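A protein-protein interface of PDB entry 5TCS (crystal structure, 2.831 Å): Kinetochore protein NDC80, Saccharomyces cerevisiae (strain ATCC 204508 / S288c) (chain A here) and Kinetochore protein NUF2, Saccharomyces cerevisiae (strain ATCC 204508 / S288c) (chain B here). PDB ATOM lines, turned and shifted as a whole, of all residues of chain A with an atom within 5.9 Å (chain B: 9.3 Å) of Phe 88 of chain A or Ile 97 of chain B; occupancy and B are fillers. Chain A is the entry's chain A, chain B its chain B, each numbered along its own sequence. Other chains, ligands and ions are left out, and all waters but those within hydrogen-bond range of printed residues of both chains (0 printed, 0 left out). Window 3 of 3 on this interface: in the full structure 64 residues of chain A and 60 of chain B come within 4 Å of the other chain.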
ATOM      1  N   ASP A   5     -17.832 -32.082  -1.579  1.00  0.00           N
ATOM      2  CA  ASP A   5     -17.640 -32.997  -2.700  1.00  0.00           C
ATOM      3  C   ASP A   5     -16.695 -32.372  -3.748  1.00  0.00           C
ATOM      4  O   ASP A   5     -15.746 -33.024  -4.177  1.00  0.00           O
ATOM      5  CB  ASP A   5     -19.003 -33.391  -3.293  1.00  0.00           C
ATOM      6  CG  ASP A   5     -18.893 -34.086  -4.636  1.00  0.00           C
ATOM      7  OD1 ASP A   5     -17.907 -34.822  -4.857  1.00  0.00           O
ATOM      8  OD2 ASP A   5     -19.808 -33.909  -5.468  1.00  0.00           O
ATOM      9  N   PRO A   6     -16.945 -31.113  -4.160  1.00  0.00           N
ATOM     10  CA  PRO A   6     -15.931 -30.382  -4.938  1.00  0.00           C
ATOM     11  C   PRO A   6     -14.735 -29.845  -4.157  1.00  0.00           C
ATOM     12  O   PRO A   6     -14.097 -28.899  -4.631  1.00  0.00           O
ATOM     13  CB  PRO A   6     -16.726 -29.206  -5.520  1.00  0.00           C
ATOM     14  CG  PRO A   6     -18.105 -29.641  -5.548  1.00  0.00           C
ATOM     15  CD  PRO A   6     -18.300 -30.591  -4.423  1.00  0.00           C
ATOM     16  N   ARG A   7     -14.401 -30.400  -2.989  1.00  0.00           N
ATOM     17  CA  ARG A   7     -13.335 -29.802  -2.193  1.00  0.00           C
ATOM     18  C   ARG A   7     -12.191 -30.784  -1.958  1.00  0.00           C
ATOM     19  O   ARG A   7     -12.436 -31.983  -1.788  1.00  0.00           O
ATOM     20  CB  ARG A   7     -13.868 -29.322  -0.833  1.00  0.00           C
ATOM     21  CG  ARG A   7     -15.037 -28.355  -0.926  1.00  0.00           C
ATOM     22  CD  ARG A   7     -15.552 -27.983   0.455  1.00  0.00           C
ATOM     23  NE  ARG A   7     -16.285 -29.081   1.079  1.00  0.00           N
ATOM     24  CZ  ARG A   7     -16.678 -29.096   2.349  1.00  0.00           C
ATOM     25  NH1 ARG A   7     -16.407 -28.075   3.152  1.00  0.00           N
ATOM     26  NH2 ARG A   7     -17.343 -30.142   2.821  1.00  0.00           N
ATOM     27  N   ARG A  85     -30.128 -27.472   3.950  1.00  0.00           N
ATOM     28  CA  ARG A  85     -29.776 -27.407   2.533  1.00  0.00           C
ATOM     29  C   ARG A  85     -28.268 -27.544   2.337  1.00  0.00           C
ATOM     30  O   ARG A  85     -27.670 -26.844   1.519  1.00  0.00           O
ATOM     31  CB  ARG A  85     -30.286 -26.120   1.885  1.00  0.00           C
ATOM     32  CG  ARG A  85     -31.780 -25.914   2.018  1.00  0.00           C
ATOM     33  CD  ARG A  85     -32.396 -25.599   0.674  1.00  0.00           C
ATOM     34  NE  ARG A  85     -33.717 -24.991   0.798  1.00  0.00           N
ATOM     35  CZ  ARG A  85     -34.401 -24.472  -0.218  1.00  0.00           C
ATOM     36  NH1 ARG A  85     -33.890 -24.483  -1.446  1.00  0.00           N
ATOM     37  NH2 ARG A  85     -35.597 -23.938  -0.007  1.00  0.00           N
ATOM     38  N   TYR A  86     -27.654 -28.444   3.098  1.00  0.00           N
ATOM     39  CA  TYR A  86     -26.240 -28.742   2.948  1.00  0.00           C
ATOM     40  C   TYR A  86     -25.927 -29.014   1.477  1.00  0.00           C
ATOM     41  O   TYR A  86     -26.467 -29.972   0.905  1.00  0.00           O
ATOM     42  CB  TYR A  86     -25.868 -29.951   3.803  1.00  0.00           C
ATOM     43  CG  TYR A  86     -24.383 -30.235   3.876  1.00  0.00           C
ATOM     44  CD1 TYR A  86     -23.491 -29.271   4.326  1.00  0.00           C
ATOM     45  CD2 TYR A  86     -23.875 -31.478   3.520  1.00  0.00           C
ATOM     46  CE1 TYR A  86     -22.136 -29.530   4.402  1.00  0.00           C
ATOM     47  CE2 TYR A  86     -22.524 -31.746   3.595  1.00  0.00           C
ATOM     48  CZ  TYR A  86     -21.658 -30.769   4.036  1.00  0.00           C
ATOM     49  OH  TYR A  86     -20.307 -31.031   4.112  1.00  0.00           O
ATOM     50  N   PRO A  87     -25.078 -28.207   0.833  1.00  0.00           N
ATOM     51  CA  PRO A  87     -24.874 -28.384  -0.613  1.00  0.00           C
ATOM     52  C   PRO A  87     -24.212 -29.702  -0.973  1.00  0.00           C
ATOM     53  O   PRO A  87     -24.518 -30.266  -2.031  1.00  0.00           O
ATOM     54  CB  PRO A  87     -23.994 -27.185  -0.992  1.00  0.00           C
ATOM     55  CG  PRO A  87     -23.274 -26.844   0.252  1.00  0.00           C
ATOM     56  CD  PRO A  87     -24.205 -27.158   1.386  1.00  0.00           C
ATOM     57  N   PHE A  88     -23.321 -30.212  -0.125  1.00  0.00           N
ATOM     58  CA  PHE A  88     -22.612 -31.456  -0.381  1.00  0.00           C
ATOM     59  C   PHE A  88     -23.344 -32.666   0.187  1.00  0.00           C
ATOM     60  O   PHE A  88     -22.715 -33.701   0.445  1.00  0.00           O
ATOM     61  CB  PHE A  88     -21.199 -31.372   0.196  1.00  0.00           C
ATOM     62  CG  PHE A  88     -20.545 -30.035  -0.010  1.00  0.00           C
ATOM     63  CD1 PHE A  88     -20.515 -29.452  -1.266  1.00  0.00           C
ATOM     64  CD2 PHE A  88     -19.979 -29.354   1.055  1.00  0.00           C
ATOM     65  CE1 PHE A  88     -19.923 -28.222  -1.457  1.00  0.00           C
ATOM     66  CE2 PHE A  88     -19.385 -28.122   0.867  1.00  0.00           C
ATOM     67  CZ  PHE A  88     -19.357 -27.556  -0.390  1.00  0.00           C
ATOM     68  N   LEU A  89     -24.658 -32.556   0.386  1.00  0.00           N
ATOM     69  CA  LEU A  89     -25.418 -33.634   1.010  1.00  0.00           C
ATOM     70  C   LEU A  89     -25.312 -34.929   0.214  1.00  0.00           C
ATOM     71  O   LEU A  89     -25.255 -36.020   0.794  1.00  0.00           O
ATOM     72  CB  LEU A  89     -26.879 -33.208   1.156  1.00  0.00           C
ATOM     73  CG  LEU A  89     -27.866 -34.231   1.717  1.00  0.00           C
ATOM     74  CD1 LEU A  89     -27.406 -34.749   3.069  1.00  0.00           C
ATOM     75  CD2 LEU A  89     -29.247 -33.605   1.823  1.00  0.00           C
ATOM     76  N   GLU A  90     -25.278 -34.833  -1.118  1.00  0.00           N
ATOM     77  CA  GLU A  90     -25.299 -36.034  -1.946  1.00  0.00           C
ATOM     78  C   GLU A  90     -24.107 -36.941  -1.664  1.00  0.00           C
ATOM     79  O   GLU A  90     -24.208 -38.163  -1.817  1.00  0.00           O
ATOM     80  CB  GLU A  90     -25.327 -35.653  -3.428  1.00  0.00           C
ATOM     81  CG  GLU A  90     -26.418 -34.657  -3.797  1.00  0.00           C
ATOM     82  CD  GLU A  90     -25.905 -33.231  -3.880  1.00  0.00           C
ATOM     83  OE1 GLU A  90     -25.130 -32.932  -4.814  1.00  0.00           O
ATOM     84  OE2 GLU A  90     -26.270 -32.410  -3.011  1.00  0.00           O
ATOM     85  N   SER A  91     -22.976 -36.369  -1.250  1.00  0.00           N
ATOM     86  CA  SER A  91     -21.742 -37.123  -1.060  1.00  0.00           C
ATOM     87  C   SER A  91     -21.691 -37.867   0.268  1.00  0.00           C
ATOM     88  O   SER A  91     -20.596 -38.245   0.706  1.00  0.00           O
ATOM     89  CB  SER A  91     -20.538 -36.185  -1.165  1.00  0.00           C
ATOM     90  OG  SER A  91     -20.476 -35.306  -0.055  1.00  0.00           O
ATOM     91  N   ILE A  92     -22.830 -38.098   0.915  1.00  0.00           N
ATOM     92  CA  ILE A  92     -22.872 -38.677   2.251  1.00  0.00           C
ATOM     93  C   ILE A  92     -23.899 -39.798   2.262  1.00  0.00           C
ATOM     94  O   ILE A  92     -25.048 -39.599   1.852  1.00  0.00           O
ATOM     95  CB  ILE A  92     -23.206 -37.612   3.314  1.00  0.00           C
ATOM     96  CG1 ILE A  92     -21.955 -36.781   3.611  1.00  0.00           C
ATOM     97  CG2 ILE A  92     -23.765 -38.251   4.594  1.00  0.00           C
ATOM     98  CD1 ILE A  92     -22.176 -35.643   4.571  1.00  0.00           C
ATOM     99  N   TRP A 114     -17.707 -26.549   7.199  1.00  0.00           N
ATOM    100  CA  TRP A 114     -18.803 -25.868   6.526  1.00  0.00           C
ATOM    101  C   TRP A 114     -19.770 -25.242   7.521  1.00  0.00           C
ATOM    102  O   TRP A 114     -20.333 -24.175   7.252  1.00  0.00           O
ATOM    103  CB  TRP A 114     -19.553 -26.838   5.614  1.00  0.00           C
ATOM    104  CG  TRP A 114     -20.769 -26.223   5.002  1.00  0.00           C
ATOM    105  CD1 TRP A 114     -20.819 -25.451   3.878  1.00  0.00           C
ATOM    106  CD2 TRP A 114     -22.113 -26.318   5.485  1.00  0.00           C
ATOM    107  NE1 TRP A 114     -22.112 -25.062   3.630  1.00  0.00           N
ATOM    108  CE2 TRP A 114     -22.927 -25.582   4.601  1.00  0.00           C
ATOM    109  CE3 TRP A 114     -22.709 -26.957   6.576  1.00  0.00           C
ATOM    110  CZ2 TRP A 114     -24.303 -25.467   4.775  1.00  0.00           C
ATOM    111  CZ3 TRP A 114     -24.077 -26.842   6.747  1.00  0.00           C
ATOM    112  CH2 TRP A 114     -24.858 -26.103   5.851  1.00  0.00           C
ATOM    113  N   GLN B  91     -17.683 -11.265  -4.442  1.00  0.00           N
ATOM    114  CA  GLN B  91     -17.518 -12.650  -4.017  1.00  0.00           C
ATOM    115  C   GLN B  91     -18.858 -13.273  -3.638  1.00  0.00           C
ATOM    116  O   GLN B  91     -18.901 -14.240  -2.871  1.00  0.00           O
ATOM    117  CB  GLN B  91     -16.528 -12.723  -2.851  1.00  0.00           C
ATOM    118  CG  GLN B  91     -16.122 -14.134  -2.420  1.00  0.00           C
ATOM    119  CD  GLN B  91     -14.986 -14.140  -1.415  1.00  0.00           C
ATOM    120  OE1 GLN B  91     -14.420 -13.096  -1.092  1.00  0.00           O
ATOM    121  NE2 GLN B  91     -14.656 -15.319  -0.903  1.00  0.00           N
ATOM    122  N   GLU B  92     -19.956 -12.742  -4.174  1.00  0.00           N
ATOM    123  CA  GLU B  92     -21.295 -13.134  -3.758  1.00  0.00           C
ATOM    124  C   GLU B  92     -22.056 -13.936  -4.801  1.00  0.00           C
ATOM    125  O   GLU B  92     -22.934 -14.718  -4.434  1.00  0.00           O
ATOM    126  CB  GLU B  92     -22.116 -11.890  -3.398  1.00  0.00           C
ATOM    127  CG  GLU B  92     -21.454 -10.997  -2.356  1.00  0.00           C
ATOM    128  CD  GLU B  92     -22.243  -9.732  -2.080  1.00  0.00           C
ATOM    129  OE1 GLU B  92     -23.302  -9.539  -2.712  1.00  0.00           O
ATOM    130  OE2 GLU B  92     -21.800  -8.931  -1.232  1.00  0.00           O
ATOM    131  N   GLU B  93     -21.744 -13.766  -6.089  1.00  0.00           N
ATOM    132  CA  GLU B  93     -22.476 -14.490  -7.122  1.00  0.00           C
ATOM    133  C   GLU B  93     -22.103 -15.967  -7.151  1.00  0.00           C
ATOM    134  O   GLU B  93     -22.915 -16.801  -7.568  1.00  0.00           O
ATOM    135  CB  GLU B  93     -22.223 -13.865  -8.495  1.00  0.00           C
ATOM    136  CG  GLU B  93     -22.387 -12.350  -8.534  1.00  0.00           C
ATOM    137  CD  GLU B  93     -22.842 -11.835  -9.892  1.00  0.00           C
ATOM    138  OE1 GLU B  93     -23.341 -12.638 -10.708  1.00  0.00           O
ATOM    139  OE2 GLU B  93     -22.698 -10.620 -10.141  1.00  0.00           O
ATOM    140  N   ASN B  94     -20.891 -16.311  -6.716  1.00  0.00           N
ATOM    141  CA  ASN B  94     -20.403 -17.680  -6.829  1.00  0.00           C
ATOM    142  C   ASN B  94     -20.642 -18.510  -5.576  1.00  0.00           C
ATOM    143  O   ASN B  94     -20.789 -19.733  -5.678  1.00  0.00           O
ATOM    144  CB  ASN B  94     -18.907 -17.677  -7.155  1.00  0.00           C
ATOM    145  CG  ASN B  94     -18.617 -17.173  -8.556  1.00  0.00           C
ATOM    146  OD1 ASN B  94     -19.468 -17.244  -9.443  1.00  0.00           O
ATOM    147  ND2 ASN B  94     -17.409 -16.661  -8.763  1.00  0.00           N
ATOM    148  N   GLU B  95     -20.684 -17.887  -4.397  1.00  0.00           N
ATOM    149  CA  GLU B  95     -20.862 -18.628  -3.147  1.00  0.00           C
ATOM    150  C   GLU B  95     -22.340 -18.959  -2.919  1.00  0.00           C
ATOM    151  O   GLU B  95     -22.979 -18.532  -1.957  1.00  0.00           O
ATOM    152  CB  GLU B  95     -20.265 -17.852  -1.979  1.00  0.00           C
ATOM    153  CG  GLU B  95     -18.828 -18.258  -1.664  1.00  0.00           C
ATOM    154  CD  GLU B  95     -18.243 -17.504  -0.485  1.00  0.00           C
ATOM    155  OE1 GLU B  95     -17.821 -18.159   0.492  1.00  0.00           O
ATOM    156  OE2 GLU B  95     -18.211 -16.256  -0.531  1.00  0.00           O
ATOM    157  N   ASN B  96     -22.881 -19.741  -3.856  1.00  0.00           N
ATOM    158  CA  ASN B  96     -24.149 -20.427  -3.643  1.00  0.00           C
ATOM    159  C   ASN B  96     -24.066 -21.378  -2.455  1.00  0.00           C
ATOM    160  O   ASN B  96     -25.095 -21.712  -1.860  1.00  0.00           O
ATOM    161  CB  ASN B  96     -24.524 -21.173  -4.933  1.00  0.00           C
ATOM    162  CG  ASN B  96     -25.856 -21.909  -4.848  1.00  0.00           C
ATOM    163  OD1 ASN B  96     -26.261 -22.394  -3.794  1.00  0.00           O
ATOM    164  ND2 ASN B  96     -26.537 -22.004  -5.983  1.00  0.00           N
ATOM    165  N   ILE B  97     -22.851 -21.785  -2.078  1.00  0.00           N
ATOM    166  CA  ILE B  97     -22.648 -22.779  -1.027  1.00  0.00           C
ATOM    167  C   ILE B  97     -23.399 -22.422   0.247  1.00  0.00           C
ATOM    168  O   ILE B  97     -23.842 -23.312   0.984  1.00  0.00           O
ATOM    169  CB  ILE B  97     -21.134 -22.936  -0.763  1.00  0.00           C
ATOM    170  CG1 ILE B  97     -20.424 -23.458  -2.017  1.00  0.00           C
ATOM    171  CG2 ILE B  97     -20.866 -23.849   0.431  1.00  0.00           C
ATOM    172  CD1 ILE B  97     -20.921 -24.812  -2.508  1.00  0.00           C
ATOM    173  N   TYR B  98     -23.551 -21.130   0.539  1.00  0.00           N
ATOM    174  CA  TYR B  98     -24.173 -20.701   1.783  1.00  0.00           C
ATOM    175  C   TYR B  98     -25.490 -19.962   1.609  1.00  0.00           C
ATOM    176  O   TYR B  98     -26.254 -19.890   2.572  1.00  0.00           O
ATOM    177  CB  TYR B  98     -23.221 -19.793   2.579  1.00  0.00           C
ATOM    178  CG  TYR B  98     -21.853 -20.387   2.819  1.00  0.00           C
ATOM    179  CD1 TYR B  98     -20.827 -20.201   1.903  1.00  0.00           C
ATOM    180  CD2 TYR B  98     -21.583 -21.134   3.961  1.00  0.00           C
ATOM    181  CE1 TYR B  98     -19.575 -20.738   2.112  1.00  0.00           C
ATOM    182  CE2 TYR B  98     -20.328 -21.678   4.178  1.00  0.00           C
ATOM    183  CZ  TYR B  98     -19.330 -21.474   3.250  1.00  0.00           C
ATOM    184  OH  TYR B  98     -18.079 -22.010   3.457  1.00  0.00           O
ATOM    185  N   LEU B  99     -25.786 -19.422   0.426  1.00  0.00           N
ATOM    186  CA  LEU B  99     -26.924 -18.519   0.289  1.00  0.00           C
ATOM    187  C   LEU B  99     -28.221 -19.174   0.760  1.00  0.00           C
ATOM    188  O   LEU B  99     -28.889 -18.673   1.671  1.00  0.00           O
ATOM    189  CB  LEU B  99     -27.048 -18.049  -1.161  1.00  0.00           C
ATOM    190  CG  LEU B  99     -28.273 -17.186  -1.477  1.00  0.00           C
ATOM    191  CD1 LEU B  99     -28.438 -16.053  -0.471  1.00  0.00           C
ATOM    192  CD2 LEU B  99     -28.171 -16.629  -2.884  1.00  0.00           C
ATOM    193  N   ASP B 100     -28.599 -20.296   0.142  1.00  0.00           N
ATOM    194  CA  ASP B 100     -29.855 -20.953   0.497  1.00  0.00           C
ATOM    195  C   ASP B 100     -29.909 -21.268   1.988  1.00  0.00           C
ATOM    196  O   ASP B 100     -30.880 -20.923   2.678  1.00  0.00           O
ATOM    197  CB  ASP B 100     -30.027 -22.228  -0.330  1.00  0.00           C
ATOM    198  CG  ASP B 100     -30.249 -21.941  -1.801  1.00  0.00           C
ATOM    199  OD1 ASP B 100     -30.127 -20.765  -2.200  1.00  0.00           O
ATOM    200  OD2 ASP B 100     -30.536 -22.892  -2.558  1.00  0.00           O
ATOM    201  N   THR B 101     -28.871 -21.931   2.502  1.00  0.00           N
ATOM    202  CA  THR B 101     -28.792 -22.227   3.929  1.00  0.00           C
ATOM    203  C   THR B 101     -29.064 -20.979   4.764  1.00  0.00           C
ATOM    204  O   THR B 101     -29.825 -21.019   5.739  1.00  0.00           O
ATOM    205  CB  THR B 101     -27.411 -22.801   4.258  1.00  0.00           C
ATOM    206  OG1 THR B 101     -27.173 -23.977   3.471  1.00  0.00           O
ATOM    207  CG2 THR B 101     -27.298 -23.156   5.738  1.00  0.00           C
ATOM    208  N   LEU B 102     -28.447 -19.857   4.389  1.00  0.00           N
ATOM    209  CA  LEU B 102     -28.535 -18.651   5.203  1.00  0.00           C
ATOM    210  C   LEU B 102     -29.930 -18.044   5.148  1.00  0.00           C
ATOM    211  O   LEU B 102     -30.472 -17.650   6.182  1.00  0.00           O
ATOM    212  CB  LEU B 102     -27.486 -17.633   4.754  1.00  0.00           C
ATOM    213  CG  LEU B 102     -26.021 -18.020   4.995  1.00  0.00           C
ATOM    214  CD1 LEU B 102     -25.086 -16.997   4.371  1.00  0.00           C
ATOM    215  CD2 LEU B 102     -25.717 -18.179   6.477  1.00  0.00           C
ATOM    216  N   ASN B 103     -30.527 -17.949   3.958  1.00  0.00           N
ATOM    217  CA  ASN B 103     -31.910 -17.487   3.877  1.00  0.00           C
ATOM    218  C   ASN B 103     -32.807 -18.337   4.766  1.00  0.00           C
ATOM    219  O   ASN B 103     -33.604 -17.819   5.561  1.00  0.00           O
ATOM    220  CB  ASN B 103     -32.396 -17.530   2.429  1.00  0.00           C
ATOM    221  CG  ASN B 103     -31.625 -16.589   1.527  1.00  0.00           C
ATOM    222  OD1 ASN B 103     -31.065 -15.593   1.985  1.00  0.00           O
ATOM    223  ND2 ASN B 103     -31.596 -16.898   0.234  1.00  0.00           N
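OD2 of Asp 100 of chain B lies within salt-bridge range of NH1 of Arg 85 of chain A (3.9 Å).
O of Phe 88 of chain A sits at hydrogen-bond distance from OG of Ser 91 of chain A (2.8 Å).
OG1 of Thr 101 of chain B touches O of Arg 85 of chain A, at 3.5 Å.
Pro 87 of chain A touches Ile 97 of chain B (CG to O, 3.7 Å).
Phe 88 of chain A touches Ile 97 of chain B.
NE1 of Trp 114 of chain A touches O of Ile 97 of chain B, at 3.6 Å.
Tyr 98 of chain B touches Trp 114 of chain A.
OG1 of Thr 101 of chain B touches CZ2 of Trp 114 of chain A (3.5 Å).
No residue of chain B comes within 4 Å of Ser 91 of chain A.
Of the printed residues of chain A, Thr 101 of chain B touches Arg 85 and Trp 114.
Of the printed residues of chain B, Trp 114 of chain A touches Ile 97, Tyr 98 and Thr 101.
Printed residues of chain A within 4 Å of Tyr 98 of chain B: Trp 114 (3.8 Å).
Of the printed residues of chain A, Asp 100 of chain B touches Arg 85 (3.9 Å).
Ile 92 of chain A touches none of the printed residues of chain B.
Asn 94 of chain B touches none of the printed residues of chain A.
The nearest residue of chain B that does not touch Phe 88 of chain A is Tyr 98 of chain B (6.8 Å).
The nearest residue of chain A that does not touch Ile 97 of chain B is Arg 85 of chain A (5.2 Å).
Among the printed residues, 7 pairs touch across the chains.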
